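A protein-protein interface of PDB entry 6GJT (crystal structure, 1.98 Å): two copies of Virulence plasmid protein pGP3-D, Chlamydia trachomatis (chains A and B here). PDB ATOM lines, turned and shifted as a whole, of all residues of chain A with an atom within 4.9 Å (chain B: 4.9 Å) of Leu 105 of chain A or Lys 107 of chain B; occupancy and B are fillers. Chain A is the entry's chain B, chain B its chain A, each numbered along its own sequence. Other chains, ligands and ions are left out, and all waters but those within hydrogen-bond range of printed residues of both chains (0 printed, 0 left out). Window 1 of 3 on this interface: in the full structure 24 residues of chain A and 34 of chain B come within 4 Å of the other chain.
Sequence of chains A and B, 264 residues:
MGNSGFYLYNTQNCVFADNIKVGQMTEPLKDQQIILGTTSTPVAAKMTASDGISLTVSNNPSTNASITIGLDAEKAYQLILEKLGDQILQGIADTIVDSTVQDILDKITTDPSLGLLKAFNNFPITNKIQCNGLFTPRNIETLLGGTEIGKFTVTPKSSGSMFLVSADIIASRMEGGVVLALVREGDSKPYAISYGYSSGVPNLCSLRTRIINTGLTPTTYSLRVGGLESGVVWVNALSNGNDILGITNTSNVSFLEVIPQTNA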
ATOM      1  N   VAL A 101      -0.148   9.902 -24.311  1.00  0.00           N
ATOM      2  CA  VAL A 101      -0.702   8.869 -23.461  1.00  0.00           C
ATOM      3  C   VAL A 101      -0.885   7.605 -24.294  1.00  0.00           C
ATOM      4  O   VAL A 101      -0.306   6.574 -23.953  1.00  0.00           O
ATOM      5  CB  VAL A 101      -2.024   9.335 -22.809  1.00  0.00           C
ATOM      6  CG1 VAL A 101      -2.888   8.161 -22.363  1.00  0.00           C
ATOM      7  CG2 VAL A 101      -1.729  10.267 -21.636  1.00  0.00           C
ATOM      8  N   GLN A 102      -1.670   7.682 -25.370  1.00  0.00           N
ATOM      9  CA  GLN A 102      -1.809   6.533 -26.287  1.00  0.00           C
ATOM     10  C   GLN A 102      -0.449   6.020 -26.769  1.00  0.00           C
ATOM     11  O   GLN A 102      -0.324   4.840 -27.043  1.00  0.00           O
ATOM     12  CB  GLN A 102      -2.799   6.714 -27.452  1.00  0.00           C
ATOM     13  CG  GLN A 102      -3.854   5.626 -27.555  1.00  0.00           C
ATOM     14  CD  GLN A 102      -5.168   5.936 -26.847  1.00  0.00           C
ATOM     15  OE1 GLN A 102      -5.204   6.191 -25.640  1.00  0.00           O
ATOM     16  NE2 GLN A 102      -6.266   5.886 -27.598  1.00  0.00           N
ATOM     17  N   ASP A 103       0.576   6.870 -26.837  1.00  0.00           N
ATOM     18  CA  ASP A 103       1.874   6.424 -27.359  1.00  0.00           C
ATOM     19  C   ASP A 103       2.601   5.537 -26.355  1.00  0.00           C
ATOM     20  O   ASP A 103       3.304   4.603 -26.742  1.00  0.00           O
ATOM     21  CB  ASP A 103       2.745   7.612 -27.717  1.00  0.00           C
ATOM     22  CG  ASP A 103       2.153   8.455 -28.823  1.00  0.00           C
ATOM     23  OD1 ASP A 103       1.263   7.978 -29.560  1.00  0.00           O
ATOM     24  OD2 ASP A 103       2.593   9.608 -28.963  1.00  0.00           O
ATOM     25  N   ILE A 104       2.412   5.809 -25.068  1.00  0.00           N
ATOM     26  CA  ILE A 104       2.931   4.940 -24.035  1.00  0.00           C
ATOM     27  C   ILE A 104       2.068   3.674 -23.996  1.00  0.00           C
ATOM     28  O   ILE A 104       2.572   2.546 -24.029  1.00  0.00           O
ATOM     29  CB  ILE A 104       2.897   5.648 -22.662  1.00  0.00           C
ATOM     30  CG1 ILE A 104       4.102   6.571 -22.498  1.00  0.00           C
ATOM     31  CG2 ILE A 104       2.859   4.625 -21.537  1.00  0.00           C
ATOM     32  CD1 ILE A 104       3.843   7.792 -21.633  1.00  0.00           C
ATOM     33  N   LEU A 105       0.759   3.866 -23.954  1.00  0.00           N
ATOM     34  CA  LEU A 105      -0.144   2.765 -23.836  1.00  0.00           C
ATOM     35  C   LEU A 105       0.033   1.696 -24.884  1.00  0.00           C
ATOM     36  O   LEU A 105      -0.072   0.532 -24.562  1.00  0.00           O
ATOM     37  CB  LEU A 105      -1.573   3.226 -23.828  1.00  0.00           C
ATOM     38  CG  LEU A 105      -2.023   4.166 -22.716  1.00  0.00           C
ATOM     39  CD1 LEU A 105      -3.536   4.270 -22.790  1.00  0.00           C
ATOM     40  CD2 LEU A 105      -1.583   3.704 -21.337  1.00  0.00           C
ATOM     41  N   ASP A 106       0.285   2.070 -26.131  1.00  0.00           N
ATOM     42  CA  ASP A 106       0.623   1.060 -27.154  1.00  0.00           C
ATOM     43  C   ASP A 106       1.939   0.329 -26.892  1.00  0.00           C
ATOM     44  O   ASP A 106       2.055  -0.865 -27.171  1.00  0.00           O
ATOM     45  CB  ASP A 106       0.682   1.683 -28.545  1.00  0.00           C
ATOM     46  CG  ASP A 106      -0.550   2.485 -28.865  1.00  0.00           C
ATOM     47  OD1 ASP A 106      -1.442   2.561 -27.991  1.00  0.00           O
ATOM     48  OD2 ASP A 106      -0.625   3.039 -29.977  1.00  0.00           O
ATOM     49  N   LYS A 107       2.940   1.049 -26.400  1.00  0.00           N
ATOM     50  CA  LYS A 107       4.182   0.413 -26.001  1.00  0.00           C
ATOM     51  C   LYS A 107       3.915  -0.612 -24.895  1.00  0.00           C
ATOM     52  O   LYS A 107       4.239  -1.806 -25.046  1.00  0.00           O
ATOM     53  CB  LYS A 107       5.195   1.464 -25.498  1.00  0.00           C
ATOM     54  CG  LYS A 107       6.100   2.067 -26.572  1.00  0.00           C
ATOM     55  CD  LYS A 107       7.051   1.090 -27.220  1.00  0.00           C
ATOM     56  CE  LYS A 107       8.256   1.743 -27.857  1.00  0.00           C
ATOM     57  NZ  LYS A 107       8.391   1.431 -29.304  1.00  0.00           N
ATOM     58  N   ILE A 108       3.314  -0.127 -23.805  1.00  0.00           N
ATOM     59  CA  ILE A 108       3.147  -0.922 -22.583  1.00  0.00           C
ATOM     60  C   ILE A 108       2.297  -2.158 -22.809  1.00  0.00           C
ATOM     61  O   ILE A 108       2.605  -3.203 -22.270  1.00  0.00           O
ATOM     62  CB  ILE A 108       2.725  -0.134 -21.315  1.00  0.00           C
ATOM     63  CG1 ILE A 108       1.346   0.467 -21.434  1.00  0.00           C
ATOM     64  CG2 ILE A 108       3.753   0.927 -20.978  1.00  0.00           C
ATOM     65  CD1 ILE A 108       0.866   1.047 -20.129  1.00  0.00           C
ATOM     66  N   THR A 109       1.291  -2.067 -23.673  1.00  0.00           N
ATOM     67  CA  THR A 109       0.416  -3.195 -23.949  1.00  0.00           C
ATOM     68  C   THR A 109       0.882  -4.068 -25.129  1.00  0.00           C
ATOM     69  O   THR A 109       0.167  -5.003 -25.521  1.00  0.00           O
ATOM     70  CB  THR A 109      -1.038  -2.727 -24.172  1.00  0.00           C
ATOM     71  OG1 THR A 109      -1.100  -1.883 -25.327  1.00  0.00           O
ATOM     72  CG2 THR A 109      -1.539  -1.995 -22.952  1.00  0.00           C
ATOM     73  N   ASP B 103      -1.386  11.510 -15.141  1.00  0.00           N
ATOM     74  CA  ASP B 103      -2.483  11.225 -16.049  1.00  0.00           C
ATOM     75  C   ASP B 103      -2.446   9.770 -16.480  1.00  0.00           C
ATOM     76  O   ASP B 103      -3.479   9.196 -16.752  1.00  0.00           O
ATOM     77  CB  ASP B 103      -2.508  12.111 -17.293  1.00  0.00           C
ATOM     78  CG  ASP B 103      -3.937  12.590 -17.630  1.00  0.00           C
ATOM     79  OD1 ASP B 103      -4.502  13.303 -16.783  1.00  0.00           O
ATOM     80  OD2 ASP B 103      -4.517  12.270 -18.705  1.00  0.00           O
ATOM     81  N   ILE B 104      -1.251   9.190 -16.592  1.00  0.00           N
ATOM     82  CA  ILE B 104      -1.103   7.765 -16.890  1.00  0.00           C
ATOM     83  C   ILE B 104      -1.481   6.997 -15.626  1.00  0.00           C
ATOM     84  O   ILE B 104      -2.273   6.091 -15.664  1.00  0.00           O
ATOM     85  CB  ILE B 104       0.339   7.397 -17.330  1.00  0.00           C
ATOM     86  CG1 ILE B 104       0.531   7.555 -18.847  1.00  0.00           C
ATOM     87  CG2 ILE B 104       0.662   5.950 -17.011  1.00  0.00           C
ATOM     88  CD1 ILE B 104       0.234   8.932 -19.414  1.00  0.00           C
ATOM     89  N   LEU B 105      -0.913   7.403 -14.509  1.00  0.00           N
ATOM     90  CA  LEU B 105      -1.120   6.780 -13.243  1.00  0.00           C
ATOM     91  C   LEU B 105      -2.598   6.575 -12.924  1.00  0.00           C
ATOM     92  O   LEU B 105      -2.995   5.512 -12.454  1.00  0.00           O
ATOM     93  CB  LEU B 105      -0.428   7.684 -12.158  1.00  0.00           C
ATOM     94  CG  LEU B 105       0.208   7.028 -10.931  1.00  0.00           C
ATOM     95  CD1 LEU B 105       0.890   8.068 -10.044  1.00  0.00           C
ATOM     96  CD2 LEU B 105      -0.812   6.234 -10.117  1.00  0.00           C
ATOM     97  N   ASP B 106      -3.417   7.587 -13.151  1.00  0.00           N
ATOM     98  CA  ASP B 106      -4.876   7.425 -12.971  1.00  0.00           C
ATOM     99  C   ASP B 106      -5.503   6.472 -13.980  1.00  0.00           C
ATOM    100  O   ASP B 106      -6.426   5.741 -13.643  1.00  0.00           O
ATOM    101  CB  ASP B 106      -5.602   8.768 -13.049  1.00  0.00           C
ATOM    102  CG  ASP B 106      -4.980   9.810 -12.156  1.00  0.00           C
ATOM    103  OD1 ASP B 106      -3.970   9.491 -11.490  1.00  0.00           O
ATOM    104  OD2 ASP B 106      -5.478  10.948 -12.135  1.00  0.00           O
ATOM    105  N   LYS B 107      -5.027   6.498 -15.217  1.00  0.00           N
ATOM    106  CA  LYS B 107      -5.479   5.538 -16.214  1.00  0.00           C
ATOM    107  C   LYS B 107      -5.141   4.115 -15.765  1.00  0.00           C
ATOM    108  O   LYS B 107      -6.013   3.271 -15.639  1.00  0.00           O
ATOM    109  CB  LYS B 107      -4.814   5.809 -17.577  1.00  0.00           C
ATOM    110  CG  LYS B 107      -5.621   6.679 -18.539  1.00  0.00           C
ATOM    111  CD  LYS B 107      -5.211   6.403 -20.015  1.00  0.00           C
ATOM    112  CE  LYS B 107      -6.324   5.458 -20.651  1.00  0.00           C
ATOM    113  NZ  LYS B 107      -7.662   6.079 -20.984  1.00  0.00           N
ATOM    114  N   ILE B 108      -3.866   3.884 -15.470  1.00  0.00           N
ATOM    115  CA  ILE B 108      -3.354   2.556 -15.133  1.00  0.00           C
ATOM    116  C   ILE B 108      -4.051   1.921 -13.937  1.00  0.00           C
ATOM    117  O   ILE B 108      -4.304   0.731 -13.937  1.00  0.00           O
ATOM    118  CB  ILE B 108      -1.845   2.599 -14.811  1.00  0.00           C
ATOM    119  CG1 ILE B 108      -1.043   2.793 -16.115  1.00  0.00           C
ATOM    120  CG2 ILE B 108      -1.438   1.398 -13.947  1.00  0.00           C
ATOM    121  CD1 ILE B 108      -1.091   1.686 -17.143  1.00  0.00           C
ATOM    122  N   THR B 109      -4.328   2.726 -12.920  1.00  0.00           N
ATOM    123  CA  THR B 109      -4.941   2.249 -11.687  1.00  0.00           C
ATOM    124  C   THR B 109      -6.446   2.211 -11.740  1.00  0.00           C
ATOM    125  O   THR B 109      -7.068   1.944 -10.723  1.00  0.00           O
ATOM    126  CB  THR B 109      -4.629   3.192 -10.476  1.00  0.00           C
ATOM    127  OG1 THR B 109      -3.264   3.631 -10.511  1.00  0.00           O
ATOM    128  CG2 THR B 109      -4.906   2.539  -9.097  1.00  0.00           C
ATOM    129  N   THR B 110      -7.048   2.567 -12.869  1.00  0.00           N
ATOM    130  CA  THR B 110      -8.512   2.589 -12.945  1.00  0.00           C
ATOM    131  C   THR B 110      -9.098   2.158 -14.274  1.00  0.00           C
ATOM    132  O   THR B 110     -10.310   2.009 -14.346  1.00  0.00           O
ATOM    133  CB  THR B 110      -9.101   4.007 -12.648  1.00  0.00           C
ATOM    134  OG1 THR B 110      -8.792   4.880 -13.737  1.00  0.00           O
ATOM    135  CG2 THR B 110      -8.574   4.633 -11.351  1.00  0.00           C
ATOM    136  N   ASP B 111      -8.275   1.965 -15.305  1.00  0.00           N
ATOM    137  CA  ASP B 111      -8.751   1.529 -16.613  1.00  0.00           C
ATOM    138  C   ASP B 111      -8.768  -0.003 -16.645  1.00  0.00           C
ATOM    139  O   ASP B 111      -7.743  -0.680 -16.686  1.00  0.00           O
ATOM    140  CB  ASP B 111      -7.874   2.040 -17.766  1.00  0.00           C
ATOM    141  CG  ASP B 111      -8.512   1.834 -19.129  1.00  0.00           C
ATOM    142  OD1 ASP B 111      -9.541   1.120 -19.253  1.00  0.00           O
ATOM    143  OD2 ASP B 111      -7.955   2.372 -20.106  1.00  0.00           O
ATOM    144  N   LEU B 114      -7.059  -2.156 -19.956  1.00  0.00           N
ATOM    145  CA  LEU B 114      -5.652  -2.336 -20.086  1.00  0.00           C
ATOM    146  C   LEU B 114      -5.484  -3.635 -19.358  1.00  0.00           C
ATOM    147  O   LEU B 114      -5.937  -3.803 -18.194  1.00  0.00           O
ATOM    148  CB  LEU B 114      -4.848  -1.302 -19.303  1.00  0.00           C
ATOM    149  CG  LEU B 114      -5.075   0.166 -19.708  1.00  0.00           C
ATOM    150  CD1 LEU B 114      -4.353   1.124 -18.770  1.00  0.00           C
ATOM    151  CD2 LEU B 114      -4.637   0.380 -21.152  1.00  0.00           C
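Of the printed residues of chain B, Val 101 of chain A touches Ile 104 and Lys 107.
Leu 105 of chain A touches just one residue of chain B: Lys 107.
Asp 106 of chain A touches none of the printed residues of chain B.
Printed residues of chain B within 4 Å of Ile 108 of chain A: Ile 108.
Of the printed residues of chain A, Ile 104 of chain B touches Val 101 (3.3 Å).
Printed residues of chain A within 4 Å of Lys 107 of chain B: Val 101 and Leu 105.
Of the printed residues of chain A, Ile 108 of chain B touches Ile 108 (3.6 Å).
Thr 109 of chain B touches none of the printed residues of chain A.
The nearest residue of chain B that does not touch Leu 105 of chain A is Leu 114 of chain B (4.4 Å).
The nearest printed residue of chain A that does not touch Lys 107 of chain B is Gln 102 of chain A (5.2 Å).
Printed residues of chain B that touch a printed residue of chain A: Ile 104, Lys 107 and Ile 108.
Among the printed residues, 4 pairs touch across the chains.
CD1 of Ile 104 of chain B touches CG2 of Val 101 of chain A, 3.3 Å away.
CG1 of Val 101 of chain A touches CD of Lys 107 of chain B, 3.7 Å away.
CE of Lys 107 of chain B touches CD1 of Leu 105 of chain A (3.7 Å).
Ile 108 of chain B touches Ile 108 of chain A (CD1 to CD1, 3.6 Å).
The side-chain amino group (NZ) of Lys 107 of chain B is in salt-bridge range of the side-chain carboxylate (OD2) of Asp 111 of chain B (3.8 Å).
The side-chain hydroxyl of Thr 109 of chain A lies within hydrogen-bond range of the backbone carbonyl oxygen of Leu 105 of chain A (2.7 Å).
Leu 105 of chain A touches Lys 107 of chain B, but with the chains exchanged Lys 107 of chain A does not touch Leu 105 of chain B (13.9 Å).
Ile 108 of chain A touches its own counterpart, Ile 108 of chain B.
7 positions are printed for both chains.
Of the 4 pairs that touch across the chains among the printed residues, 1 has its exchanged pair printed and touching as well.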
